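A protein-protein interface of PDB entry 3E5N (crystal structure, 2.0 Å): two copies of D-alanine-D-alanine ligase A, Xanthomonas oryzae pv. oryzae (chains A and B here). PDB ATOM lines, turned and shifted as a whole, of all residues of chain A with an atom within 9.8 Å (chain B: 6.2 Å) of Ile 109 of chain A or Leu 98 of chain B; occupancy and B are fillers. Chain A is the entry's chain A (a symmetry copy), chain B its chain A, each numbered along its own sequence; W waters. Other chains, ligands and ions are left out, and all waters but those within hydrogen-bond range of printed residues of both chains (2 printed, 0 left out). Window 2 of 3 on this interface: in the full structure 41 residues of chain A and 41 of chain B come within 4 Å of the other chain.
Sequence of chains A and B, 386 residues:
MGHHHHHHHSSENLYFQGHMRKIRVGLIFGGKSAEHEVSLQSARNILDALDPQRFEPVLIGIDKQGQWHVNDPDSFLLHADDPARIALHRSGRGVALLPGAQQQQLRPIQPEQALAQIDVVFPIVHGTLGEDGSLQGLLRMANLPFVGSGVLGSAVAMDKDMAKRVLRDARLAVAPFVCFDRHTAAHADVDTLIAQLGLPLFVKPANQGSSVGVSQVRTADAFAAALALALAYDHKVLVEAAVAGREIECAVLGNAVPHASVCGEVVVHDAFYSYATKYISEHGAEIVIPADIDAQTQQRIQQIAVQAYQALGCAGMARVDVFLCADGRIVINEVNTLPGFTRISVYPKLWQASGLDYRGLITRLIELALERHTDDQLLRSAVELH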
ATOM      1  N   GLY A  66      12.534   0.091  -6.064  1.00  0.00           N
ATOM      2  CA  GLY A  66      13.101   1.007  -5.079  1.00  0.00           C
ATOM      3  C   GLY A  66      14.473   1.536  -5.453  1.00  0.00           C
ATOM      4  O   GLY A  66      15.114   2.245  -4.650  1.00  0.00           O
ATOM      5  N   GLN A  67      14.903   1.265  -6.683  1.00  0.00           N
ATOM      6  CA  GLN A  67      16.190   1.713  -7.141  1.00  0.00           C
ATOM      7  C   GLN A  67      16.165   3.120  -7.722  1.00  0.00           C
ATOM      8  O   GLN A  67      15.240   3.471  -8.457  1.00  0.00           O
ATOM      9  CB  GLN A  67      16.784   0.720  -8.184  1.00  0.00           C
ATOM     10  CG  GLN A  67      16.875  -0.746  -7.715  1.00  0.00           C
ATOM     11  CD  GLN A  67      17.752  -0.988  -6.470  1.00  0.00           C
ATOM     12  OE1 GLN A  67      17.296  -1.653  -5.503  1.00  0.00           O
ATOM     13  NE2 GLN A  67      19.024  -0.481  -6.485  1.00  0.00           N
ATOM     14  N   TRP A  68      17.208   3.906  -7.417  1.00  0.00           N
ATOM     15  CA  TRP A  68      17.284   5.311  -7.777  1.00  0.00           C
ATOM     16  C   TRP A  68      18.022   5.521  -9.102  1.00  0.00           C
ATOM     17  O   TRP A  68      19.031   4.915  -9.365  1.00  0.00           O
ATOM     18  CB  TRP A  68      18.012   6.117  -6.668  1.00  0.00           C
ATOM     19  CG  TRP A  68      17.250   6.268  -5.307  1.00  0.00           C
ATOM     20  CD1 TRP A  68      16.446   5.345  -4.703  1.00  0.00           C
ATOM     21  CD2 TRP A  68      17.276   7.401  -4.429  1.00  0.00           C
ATOM     22  NE1 TRP A  68      15.949   5.849  -3.516  1.00  0.00           N
ATOM     23  CE2 TRP A  68      16.440   7.107  -3.328  1.00  0.00           C
ATOM     24  CE3 TRP A  68      17.942   8.620  -4.447  1.00  0.00           C
ATOM     25  CZ2 TRP A  68      16.251   8.012  -2.268  1.00  0.00           C
ATOM     26  CZ3 TRP A  68      17.725   9.524  -3.416  1.00  0.00           C
ATOM     27  CH2 TRP A  68      16.906   9.210  -2.338  1.00  0.00           C
ATOM     28  N   HIS A  69      17.533   6.452  -9.912  1.00  0.00           N
ATOM     29  CA  HIS A  69      18.059   6.671 -11.257  1.00  0.00           C
ATOM     30  C   HIS A  69      18.108   8.135 -11.527  1.00  0.00           C
ATOM     31  O   HIS A  69      17.040   8.790 -11.543  1.00  0.00           O
ATOM     32  CB  HIS A  69      17.116   6.071 -12.285  1.00  0.00           C
ATOM     33  CG  HIS A  69      17.068   4.583 -12.269  1.00  0.00           C
ATOM     34  ND1 HIS A  69      16.065   3.867 -11.641  1.00  0.00           N
ATOM     35  CD2 HIS A  69      17.871   3.668 -12.859  1.00  0.00           C
ATOM     36  CE1 HIS A  69      16.281   2.570 -11.809  1.00  0.00           C
ATOM     37  NE2 HIS A  69      17.354   2.425 -12.567  1.00  0.00           N
ATOM     38  N   VAL A  70      19.301   8.661 -11.756  1.00  0.00           N
ATOM     39  CA  VAL A  70      19.408  10.050 -12.213  1.00  0.00           C
ATOM     40  C   VAL A  70      19.008  10.079 -13.685  1.00  0.00           C
ATOM     41  O   VAL A  70      19.366   9.182 -14.439  1.00  0.00           O
ATOM     42  CB  VAL A  70      20.819  10.634 -12.042  1.00  0.00           C
ATOM     43  CG1 VAL A  70      20.861  12.115 -12.522  1.00  0.00           C
ATOM     44  CG2 VAL A  70      21.292  10.517 -10.593  1.00  0.00           C
ATOM     45  N   SER A  91      17.578   4.552 -16.163  1.00  0.00           N
ATOM     46  CA  SER A  91      18.877   4.848 -16.686  1.00  0.00           C
ATOM     47  C   SER A  91      20.070   4.039 -16.067  1.00  0.00           C
ATOM     48  O   SER A  91      21.139   3.943 -16.691  1.00  0.00           O
ATOM     49  CB  SER A  91      19.126   6.346 -16.487  1.00  0.00           C
ATOM     50  OG  SER A  91      19.384   6.594 -15.107  1.00  0.00           O
ATOM     51  N   GLY A  92      19.882   3.478 -14.863  1.00  0.00           N
ATOM     52  CA  GLY A  92      20.944   2.735 -14.160  1.00  0.00           C
ATOM     53  C   GLY A  92      22.026   3.682 -13.676  1.00  0.00           C
ATOM     54  O   GLY A  92      23.087   3.253 -13.174  1.00  0.00           O
ATOM     55  N   ARG A  93      21.782   4.976 -13.787  1.00  0.00           N
ATOM     56  CA  ARG A  93      22.705   5.971 -13.214  1.00  0.00           C
ATOM     57  C   ARG A  93      22.447   6.140 -11.702  1.00  0.00           C
ATOM     58  O   ARG A  93      21.555   6.891 -11.319  1.00  0.00           O
ATOM     59  CB  ARG A  93      22.520   7.313 -13.905  1.00  0.00           C
ATOM     60  CG  ARG A  93      22.938   7.271 -15.363  1.00  0.00           C
ATOM     61  CD  ARG A  93      22.319   8.425 -16.153  1.00  0.00           C
ATOM     62  NE  ARG A  93      22.810   9.689 -15.633  1.00  0.00           N
ATOM     63  CZ  ARG A  93      22.440  10.882 -16.083  1.00  0.00           C
ATOM     64  NH1 ARG A  93      21.552  11.006 -17.080  1.00  0.00           N
ATOM     65  NH2 ARG A  93      22.976  11.958 -15.528  1.00  0.00           N
ATOM     66  N   GLY A  94      23.211   5.454 -10.856  1.00  0.00           N
ATOM     67  CA  GLY A  94      22.860   5.338  -9.434  1.00  0.00           C
ATOM     68  C   GLY A  94      23.210   6.556  -8.618  1.00  0.00           C
ATOM     69  O   GLY A  94      23.988   7.385  -9.072  1.00  0.00           O
ATOM     70  N   VAL A  95      22.619   6.664  -7.419  1.00  0.00           N
ATOM     71  CA  VAL A  95      22.856   7.770  -6.494  1.00  0.00           C
ATOM     72  C   VAL A  95      23.434   7.265  -5.163  1.00  0.00           C
ATOM     73  O   VAL A  95      22.944   6.295  -4.602  1.00  0.00           O
ATOM     74  CB  VAL A  95      21.491   8.475  -6.127  1.00  0.00           C
ATOM     75  CG1 VAL A  95      21.710   9.610  -5.142  1.00  0.00           C
ATOM     76  CG2 VAL A  95      20.762   8.941  -7.386  1.00  0.00           C
ATOM     77  N   ALA A  96      24.377   7.999  -4.595  1.00  0.00           N
ATOM     78  CA  ALA A  96      24.847   7.731  -3.252  1.00  0.00           C
ATOM     79  C   ALA A  96      24.605   8.973  -2.437  1.00  0.00           C
ATOM     80  O   ALA A  96      24.651  10.085  -2.945  1.00  0.00           O
ATOM     81  CB  ALA A  96      26.301   7.450  -3.279  1.00  0.00           C
ATOM     82  N   LEU A  97      24.333   8.757  -1.165  1.00  0.00           N
ATOM     83  CA  LEU A  97      24.117   9.835  -0.229  1.00  0.00           C
ATOM     84  C   LEU A  97      25.226   9.798   0.794  1.00  0.00           C
ATOM     85  O   LEU A  97      25.596   8.739   1.299  1.00  0.00           O
ATOM     86  CB  LEU A  97      22.738   9.701   0.423  1.00  0.00           C
ATOM     87  CG  LEU A  97      21.716  10.449  -0.471  1.00  0.00           C
ATOM     88  CD1 LEU A  97      20.803   9.495  -1.274  1.00  0.00           C
ATOM     89  CD2 LEU A  97      20.892  11.410   0.366  1.00  0.00           C
ATOM     90  N   LEU A  98      25.766  10.963   1.078  1.00  0.00           N
ATOM     91  CA  LEU A  98      26.817  11.104   2.077  1.00  0.00           C
ATOM     92  C   LEU A  98      26.254  11.736   3.344  1.00  0.00           C
ATOM     93  O   LEU A  98      26.112  12.948   3.427  1.00  0.00           O
ATOM     94  CB  LEU A  98      27.950  11.937   1.530  1.00  0.00           C
ATOM     95  CG  LEU A  98      28.394  11.539   0.114  1.00  0.00           C
ATOM     96  CD1 LEU A  98      29.571  12.371  -0.297  1.00  0.00           C
ATOM     97  CD2 LEU A  98      28.755  10.099  -0.096  1.00  0.00           C
ATOM     98  N   PRO A  99      25.866  10.885   4.315  1.00  0.00           N
ATOM     99  CA  PRO A  99      25.211  11.297   5.541  1.00  0.00           C
ATOM    100  C   PRO A  99      26.200  12.222   6.196  1.00  0.00           C
ATOM    101  O   PRO A  99      27.374  11.923   6.191  1.00  0.00           O
ATOM    102  CB  PRO A  99      25.132  10.007   6.367  1.00  0.00           C
ATOM    103  CG  PRO A  99      25.567   8.955   5.543  1.00  0.00           C
ATOM    104  CD  PRO A  99      26.046   9.424   4.247  1.00  0.00           C
ATOM    105  N   GLN A 104      27.535  18.543  -2.062  1.00  0.00           N
ATOM    106  CA  GLN A 104      27.535  17.340  -2.928  1.00  0.00           C
ATOM    107  C   GLN A 104      27.091  16.134  -2.110  1.00  0.00           C
ATOM    108  O   GLN A 104      27.698  15.040  -2.142  1.00  0.00           O
ATOM    109  CB  GLN A 104      28.923  17.086  -3.499  1.00  0.00           C
ATOM    110  CG  GLN A 104      29.264  17.960  -4.678  1.00  0.00           C
ATOM    111  CD  GLN A 104      28.482  17.580  -5.923  1.00  0.00           C
ATOM    112  OE1 GLN A 104      27.948  18.462  -6.604  1.00  0.00           O
ATOM    113  NE2 GLN A 104      28.412  16.259  -6.242  1.00  0.00           N
ATOM    114  N   GLN A 105      26.045  16.338  -1.330  1.00  0.00           N
ATOM    115  CA  GLN A 105      25.510  15.222  -0.488  1.00  0.00           C
ATOM    116  C   GLN A 105      24.970  14.063  -1.278  1.00  0.00           C
ATOM    117  O   GLN A 105      25.035  12.922  -0.824  1.00  0.00           O
ATOM    118  CB  GLN A 105      24.437  15.741   0.406  1.00  0.00           C
ATOM    119  CG  GLN A 105      24.948  16.901   1.221  1.00  0.00           C
ATOM    120  CD  GLN A 105      24.474  18.144   0.656  1.00  0.00           C
ATOM    121  OE1 GLN A 105      24.696  18.418  -0.535  1.00  0.00           O
ATOM    122  NE2 GLN A 105      23.754  18.915   1.449  1.00  0.00           N
ATOM    123  N   LEU A 106      24.432  14.377  -2.476  1.00  0.00           N
ATOM    124  CA  LEU A 106      23.948  13.367  -3.399  1.00  0.00           C
ATOM    125  C   LEU A 106      24.962  13.197  -4.510  1.00  0.00           C
ATOM    126  O   LEU A 106      25.338  14.154  -5.204  1.00  0.00           O
ATOM    127  CB  LEU A 106      22.512  13.689  -3.895  1.00  0.00           C
ATOM    128  CG  LEU A 106      21.456  13.576  -2.788  1.00  0.00           C
ATOM    129  CD1 LEU A 106      21.442  14.870  -2.002  1.00  0.00           C
ATOM    130  CD2 LEU A 106      20.101  13.415  -3.320  1.00  0.00           C
ATOM    131  N   ARG A 107      25.475  11.984  -4.631  1.00  0.00           N
ATOM    132  CA  ARG A 107      26.605  11.706  -5.539  1.00  0.00           C
ATOM    133  C   ARG A 107      26.332  10.562  -6.463  1.00  0.00           C
ATOM    134  O   ARG A 107      25.686   9.632  -6.064  1.00  0.00           O
ATOM    135  CB  ARG A 107      27.869  11.419  -4.747  1.00  0.00           C
ATOM    136  CG  ARG A 107      28.553  12.742  -4.497  1.00  0.00           C
ATOM    137  CD  ARG A 107      29.907  12.638  -3.891  1.00  0.00           C
ATOM    138  NE  ARG A 107      30.004  13.744  -2.970  1.00  0.00           N
ATOM    139  CZ  ARG A 107      31.074  14.058  -2.258  1.00  0.00           C
ATOM    140  NH1 ARG A 107      32.189  13.326  -2.379  1.00  0.00           N
ATOM    141  NH2 ARG A 107      30.994  15.076  -1.394  1.00  0.00           N
ATOM    142  N   PRO A 108      26.785  10.655  -7.724  1.00  0.00           N
ATOM    143  CA  PRO A 108      26.642   9.549  -8.645  1.00  0.00           C
ATOM    144  C   PRO A 108      27.507   8.341  -8.286  1.00  0.00           C
ATOM    145  O   PRO A 108      28.707   8.499  -8.108  1.00  0.00           O
ATOM    146  CB  PRO A 108      27.138  10.148  -9.981  1.00  0.00           C
ATOM    147  CG  PRO A 108      28.009  11.234  -9.618  1.00  0.00           C
ATOM    148  CD  PRO A 108      27.383  11.833  -8.386  1.00  0.00           C
ATOM    149  N   ILE A 109      26.900   7.164  -8.148  1.00  0.00           N
ATOM    150  CA  ILE A 109      27.650   5.907  -8.144  1.00  0.00           C
ATOM    151  C   ILE A 109      28.190   5.897  -9.569  1.00  0.00           C
ATOM    152  O   ILE A 109      27.406   6.107 -10.519  1.00  0.00           O
ATOM    153  CB  ILE A 109      26.734   4.672  -7.884  1.00  0.00           C
ATOM    154  CG1 ILE A 109      25.965   4.822  -6.562  1.00  0.00           C
ATOM    155  CG2 ILE A 109      27.529   3.352  -7.903  1.00  0.00           C
ATOM    156  CD1 ILE A 109      24.795   3.850  -6.451  1.00  0.00           C
ATOM    157  N   GLN A 110      29.510   5.720  -9.724  1.00  0.00           N
ATOM    158  CA  GLN A 110      30.219   5.948 -11.014  1.00  0.00           C
ATOM    159  C   GLN A 110      30.759   7.373 -11.010  1.00  0.00           C
ATOM    160  O   GLN A 110      31.691   7.686 -10.267  1.00  0.00           O
ATOM    161  CB  GLN A 110      29.332   5.739 -12.268  1.00  0.00           C
ATOM    162  CG  GLN A 110      28.779   4.300 -12.522  1.00  0.00           C
ATOM    163  CD  GLN A 110      27.305   4.303 -12.998  1.00  0.00           C
ATOM    164  OE1 GLN A 110      27.004   4.568 -14.182  1.00  0.00           O
ATOM    165  NE2 GLN A 110      26.377   4.009 -12.065  1.00  0.00           N
ATOM    166  N   GLN A 113      29.905  10.157 -12.708  1.00  0.00           N
ATOM    167  CA  GLN A 113      30.969  11.047 -12.219  1.00  0.00           C
ATOM    168  C   GLN A 113      30.513  12.314 -11.439  1.00  0.00           C
ATOM    169  O   GLN A 113      30.881  12.481 -10.249  1.00  0.00           O
ATOM    170  CB  GLN A 113      31.987  11.377 -13.329  1.00  0.00           C
ATOM    171  CG  GLN A 113      31.389  11.830 -14.686  1.00  0.00           C
ATOM    172  CD  GLN A 113      30.654  10.708 -15.407  1.00  0.00           C
ATOM    173  OE1 GLN A 113      29.432  10.790 -15.636  1.00  0.00           O
ATOM    174  NE2 GLN A 113      31.381   9.638 -15.737  1.00  0.00           N
ATOM    175  N   ALA A 114      29.700  13.184 -12.054  1.00  0.00           N
ATOM    176  CA  ALA A 114      29.241  14.398 -11.324  1.00  0.00           C
ATOM    177  C   ALA A 114      27.740  14.701 -11.455  1.00  0.00           C
ATOM    178  O   ALA A 114      27.155  14.564 -12.541  1.00  0.00           O
ATOM    179  CB  ALA A 114      30.095  15.633 -11.673  1.00  0.00           C
ATOM    180  N   LEU A 115      27.139  15.076 -10.318  1.00  0.00           N
ATOM    181  CA  LEU A 115      25.714  15.477 -10.215  1.00  0.00           C
ATOM    182  C   LEU A 115      25.686  16.915  -9.743  1.00  0.00           C
ATOM    183  O   LEU A 115      26.447  17.283  -8.863  1.00  0.00           O
ATOM    184  CB  LEU A 115      24.971  14.565  -9.218  1.00  0.00           C
ATOM    185  CG  LEU A 115      23.489  14.712  -8.851  1.00  0.00           C
ATOM    186  CD1 LEU A 115      22.626  14.225  -9.967  1.00  0.00           C
ATOM    187  CD2 LEU A 115      23.159  13.916  -7.594  1.00  0.00           C
ATOM    188  N   LEU A 138      16.201  10.568   5.774  1.00  0.00           N
ATOM    189  CA  LEU A 138      17.379  10.494   4.913  1.00  0.00           C
ATOM    190  C   LEU A 138      17.795  11.910   4.469  1.00  0.00           C
ATOM    191  O   LEU A 138      18.996  12.193   4.488  1.00  0.00           O
ATOM    192  CB  LEU A 138      17.110   9.569   3.701  1.00  0.00           C
ATOM    193  CG  LEU A 138      18.205   9.508   2.577  1.00  0.00           C
ATOM    194  CD1 LEU A 138      17.992   8.398   1.638  1.00  0.00           C
ATOM    195  CD2 LEU A 138      18.157  10.799   1.639  1.00  0.00           C
ATOM    196  N   ALA B  96      29.331   6.218   2.418  1.00  0.00           N
ATOM    197  CA  ALA B  96      28.243   6.590   1.538  1.00  0.00           C
ATOM    198  C   ALA B  96      27.152   5.569   1.721  1.00  0.00           C
ATOM    199  O   ALA B  96      27.409   4.406   2.002  1.00  0.00           O
ATOM    200  CB  ALA B  96      28.704   6.551   0.131  1.00  0.00           C
ATOM    201  N   LEU B  97      25.927   6.035   1.570  1.00  0.00           N
ATOM    202  CA  LEU B  97      24.763   5.187   1.668  1.00  0.00           C
ATOM    203  C   LEU B  97      24.093   5.149   0.315  1.00  0.00           C
ATOM    204  O   LEU B  97      23.935   6.173  -0.348  1.00  0.00           O
ATOM    205  CB  LEU B  97      23.818   5.707   2.754  1.00  0.00           C
ATOM    206  CG  LEU B  97      24.239   5.059   4.099  1.00  0.00           C
ATOM    207  CD1 LEU B  97      24.960   6.045   5.046  1.00  0.00           C
ATOM    208  CD2 LEU B  97      23.035   4.435   4.780  1.00  0.00           C
ATOM    209  N   LEU B  98      23.721   3.957  -0.095  1.00  0.00           N
ATOM    210  CA  LEU B  98      23.023   3.757  -1.358  1.00  0.00           C
ATOM    211  C   LEU B  98      21.549   3.464  -1.100  1.00  0.00           C
ATOM    212  O   LEU B  98      21.181   2.337  -0.800  1.00  0.00           O
ATOM    213  CB  LEU B  98      23.657   2.629  -2.134  1.00  0.00           C
ATOM    214  CG  LEU B  98      25.191   2.698  -2.198  1.00  0.00           C
ATOM    215  CD1 LEU B  98      25.709   1.584  -3.056  1.00  0.00           C
ATOM    216  CD2 LEU B  98      25.784   3.979  -2.703  1.00  0.00           C
ATOM    217  N   PRO B  99      20.713   4.520  -1.154  1.00  0.00           N
ATOM    218  CA  PRO B  99      19.300   4.452  -0.832  1.00  0.00           C
ATOM    219  C   PRO B  99      18.745   3.454  -1.812  1.00  0.00           C
ATOM    220  O   PRO B  99      19.116   3.495  -2.964  1.00  0.00           O
ATOM    221  CB  PRO B  99      18.771   5.842  -1.203  1.00  0.00           C
ATOM    222  CG  PRO B  99      19.882   6.637  -1.536  1.00  0.00           C
ATOM    223  CD  PRO B  99      21.130   5.882  -1.533  1.00  0.00           C
ATOM    224  N   GLY B 100      17.922   2.531  -1.342  1.00  0.00           N
ATOM    225  CA  GLY B 100      17.266   1.623  -2.262  1.00  0.00           C
ATOM    226  C   GLY B 100      18.107   0.397  -2.541  1.00  0.00           C
ATOM    227  O   GLY B 100      17.593  -0.545  -3.061  1.00  0.00           O
ATOM    228  N   ALA B 101      19.400   0.425  -2.213  1.00  0.00           N
ATOM    229  CA  ALA B 101      20.289  -0.722  -2.415  1.00  0.00           C
ATOM    230  C   ALA B 101      19.865  -1.827  -1.471  1.00  0.00           C
ATOM    231  O   ALA B 101      19.233  -1.588  -0.442  1.00  0.00           O
ATOM    232  CB  ALA B 101      21.821  -0.347  -2.242  1.00  0.00           C
ATOM    233  N   GLN B 102      20.119  -3.054  -1.893  1.00  0.00           N
ATOM    234  CA  GLN B 102      19.769  -4.176  -1.076  1.00  0.00           C
ATOM    235  C   GLN B 102      20.972  -4.910  -0.524  1.00  0.00           C
ATOM    236  O   GLN B 102      20.771  -5.780   0.296  1.00  0.00           O
ATOM    237  CB  GLN B 102      18.903  -5.156  -1.848  1.00  0.00           C
ATOM    238  CG  GLN B 102      17.660  -5.529  -1.053  1.00  0.00           C
ATOM    239  CD  GLN B 102      16.462  -5.196  -1.833  1.00  0.00           C
ATOM    240  OE1 GLN B 102      16.437  -5.460  -3.043  1.00  0.00           O
ATOM    241  NE2 GLN B 102      15.470  -4.555  -1.190  1.00  0.00           N
ATOM    242  N   GLN B 103      22.194  -4.568  -0.965  1.00  0.00           N
ATOM    243  CA  GLN B 103      23.441  -5.116  -0.388  1.00  0.00           C
ATOM    244  C   GLN B 103      24.538  -4.109  -0.494  1.00  0.00           C
ATOM    245  O   GLN B 103      24.482  -3.255  -1.358  1.00  0.00           O
ATOM    246  CB  GLN B 103      23.876  -6.454  -1.034  1.00  0.00           C
ATOM    247  CG  GLN B 103      23.623  -6.580  -2.528  1.00  0.00           C
ATOM    248  CD  GLN B 103      22.910  -7.914  -2.839  1.00  0.00           C
ATOM    249  OE1 GLN B 103      23.561  -8.947  -3.065  1.00  0.00           O
ATOM    250  NE2 GLN B 103      21.567  -7.903  -2.771  1.00  0.00           N
ATOM    251  N   GLN B 104      25.550  -4.223   0.351  1.00  0.00           N
ATOM    252  CA  GLN B 104      26.620  -3.198   0.417  1.00  0.00           C
ATOM    253  C   GLN B 104      25.986  -1.811   0.406  1.00  0.00           C
ATOM    254  O   GLN B 104      26.404  -0.888  -0.329  1.00  0.00           O
ATOM    255  CB  GLN B 104      27.571  -3.333  -0.763  1.00  0.00           C
ATOM    256  CG  GLN B 104      28.587  -4.434  -0.600  1.00  0.00           C
ATOM    257  CD  GLN B 104      29.638  -4.098   0.443  1.00  0.00           C
ATOM    258  OE1 GLN B 104      29.957  -4.944   1.285  1.00  0.00           O
ATOM    259  NE2 GLN B 104      30.198  -2.858   0.396  1.00  0.00           N
ATOM    260  N   GLN B 105      24.937  -1.666   1.194  1.00  0.00           N
ATOM    261  CA  GLN B 105      24.239  -0.346   1.276  1.00  0.00           C
ATOM    262  C   GLN B 105      25.087   0.763   1.836  1.00  0.00           C
ATOM    263  O   GLN B 105      24.915   1.921   1.462  1.00  0.00           O
ATOM    264  CB  GLN B 105      23.008  -0.482   2.106  1.00  0.00           C
ATOM    265  CG  GLN B 105      22.129  -1.580   1.567  1.00  0.00           C
ATOM    266  CD  GLN B 105      22.279  -2.769   2.375  1.00  0.00           C
ATOM    267  OE1 GLN B 105      23.402  -3.267   2.559  1.00  0.00           O
ATOM    268  NE2 GLN B 105      21.182  -3.237   2.941  1.00  0.00           N
ATOM    269  N   LEU B 106      26.011   0.384   2.744  1.00  0.00           N
ATOM    270  CA  LEU B 106      26.966   1.315   3.314  1.00  0.00           C
ATOM    271  C   LEU B 106      28.313   1.092   2.658  1.00  0.00           C
ATOM    272  O   LEU B 106      28.864  -0.020   2.658  1.00  0.00           O
ATOM    273  CB  LEU B 106      26.995   1.227   4.864  1.00  0.00           C
ATOM    274  CG  LEU B 106      25.701   1.732   5.516  1.00  0.00           C
ATOM    275  CD1 LEU B 106      24.685   0.609   5.501  1.00  0.00           C
ATOM    276  CD2 LEU B 106      25.885   2.087   6.925  1.00  0.00           C
ATOM    277  N   ARG B 107      28.814   2.136   2.019  1.00  0.00           N
ATOM    278  CA  ARG B 107      30.021   2.024   1.178  1.00  0.00           C
ATOM    279  C   ARG B 107      31.061   3.040   1.527  1.00  0.00           C
ATOM    280  O   ARG B 107      30.713   4.137   1.873  1.00  0.00           O
ATOM    281  CB  ARG B 107      29.663   2.161  -0.292  1.00  0.00           C
ATOM    282  CG  ARG B 107      29.327   0.780  -0.803  1.00  0.00           C
ATOM    283  CD  ARG B 107      29.128   0.691  -2.274  1.00  0.00           C
ATOM    284  NE  ARG B 107      28.053  -0.251  -2.463  1.00  0.00           N
ATOM    285  CZ  ARG B 107      27.593  -0.667  -3.631  1.00  0.00           C
ATOM    286  NH1 ARG B 107      28.151  -0.214  -4.763  1.00  0.00           N
ATOM    287  NH2 ARG B 107      26.545  -1.497  -3.650  1.00  0.00           N
ATOM    288  N   MET B 141      15.658   3.576   4.539  1.00  0.00           N
ATOM    289  CA  MET B 141      15.921   3.848   3.094  1.00  0.00           C
ATOM    290  C   MET B 141      16.983   2.907   2.514  1.00  0.00           C
ATOM    291  O   MET B 141      16.965   2.614   1.284  1.00  0.00           O
ATOM    292  CB  MET B 141      16.382   5.311   2.834  1.00  0.00           C
ATOM    293  CG  MET B 141      15.261   6.358   2.993  1.00  0.00           C
ATOM    294  SD  MET B 141      13.638   5.956   2.226  1.00  0.00           S
ATOM    295  CE  MET B 141      14.126   5.956   0.504  1.00  0.00           C
ATOM    296  N   ALA B 142      17.893   2.470   3.377  1.00  0.00           N
ATOM    297  CA  ALA B 142      18.998   1.613   2.962  1.00  0.00           C
ATOM    298  C   ALA B 142      18.671   0.140   3.188  1.00  0.00           C
ATOM    299  O   ALA B 142      19.531  -0.717   3.005  1.00  0.00           O
ATOM    300  CB  ALA B 142      20.327   2.042   3.768  1.00  0.00           C
HETATM  301  O   HOH W   1      21.704   4.034  -4.327  1.00  0.00           O
HETATM  302  O   HOH W   2      19.072   2.656  -5.527  1.00  0.00           O
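Ala 96 of chain A touches Leu 98 of chain B, and with the chains exchanged Leu 98 of chain A touches Ala 96 of chain B. Positions printed for both chains: 96, 97, 98, 99, 104, 105, 106 and 107. Of the 14 pairs that touch across the chains among the printed residues, 7 have their exchanged pair printed and touching as well.
CE2 of Trp 68 of chain A touches CB of Pro 99 of chain B, at 3.4 Å. O of Val 95 of chain A touches CD of Pro 99 of chain B, at 3.6 Å. CG of Pro 99 of chain B touches CD1 of Leu 97 of chain A, at 3.0 Å. Leu 98 of chain A touches Ala 96 of chain B. Leu 138 of chain A touches Pro 99 of chain B (CD1 to CB, 3.9 Å). Leu 138 of chain A touches Met 141 of chain B (CD1 to CG, 3.7 Å).
Water W2 lies within hydrogen-bond range of the backbone carbonyl oxygen (O) of Pro 99 of chain B (2.7 Å), the backbone NH (N) of Trp 68 of chain A (2.9 Å) and the side-chain amide nitrogen (NE2) of Gln 67 of chain A (3.3 Å).
Of the printed residues of chain B, Ala 96 of chain A touches Leu 97 and Leu 98. Printed residues of chain B within 4 Å of Leu 98 of chain A: Ala 96. Ile 109 of chain A touches just one residue of chain B: Leu 98 (3.9 Å). Leu 97 of chain B touches just these residues of chain A: Ala 96 (3.4 Å), Leu 97 (2.7 Å) and Pro 99 (3.0 Å). Of the printed residues of chain A, Pro 99 of chain B touches Trp 68 (3.4 Å), Val 95 (3.6 Å), Leu 97 (3.0 Å) and Leu 138 (3.9 Å). No residue of chain A comes within 4 Å of Ala 101 of chain B. Gln 103 of chain B touches none of the printed residues of chain A. No residue of chain A comes within 4 Å of Ala 142 of chain B. The nearest residue of chain A that does not touch Leu 98 of chain B is Val 95 of chain A (4.1 Å).
The backbone carbonyl oxygen (O) of Gln 67 of chain A lies within hydrogen-bond range of a ring nitrogen (ND1) of His 69 of chain A, at 3.3 Å. The backbone NH (N) of Leu 98 of chain A lies within hydrogen-bond range of the backbone carbonyl oxygen (O) of Gln 105 of chain A.
The backbone carbonyl oxygen of Leu 97 of chain A sits at hydrogen-bond distance from the backbone NH of Leu 97 of chain B (2.7 Å). The side-chain amide oxygen (OE1) of Gln 67 of chain A sits close to the backbone carbonyl oxygen (O) of Gly 100 of chain B (2.7 Å).
Of the 25 printed residues of chain A, 10 touch a printed residue of chain B. Printed residues of chain A that touch a printed residue of chain B: Gly 66, Gln 67, Trp 68, Val 95, Ala 96, Leu 97, Leu 98, Pro 99, Ile 109 and Leu 138. Of the 14 printed residues of chain B, 6 touch a printed residue of chain A. Among the printed residues, no Asp or Glu carboxylate lies within 4 Å of a Lys or Arg side-chain nitrogen of the other chain.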
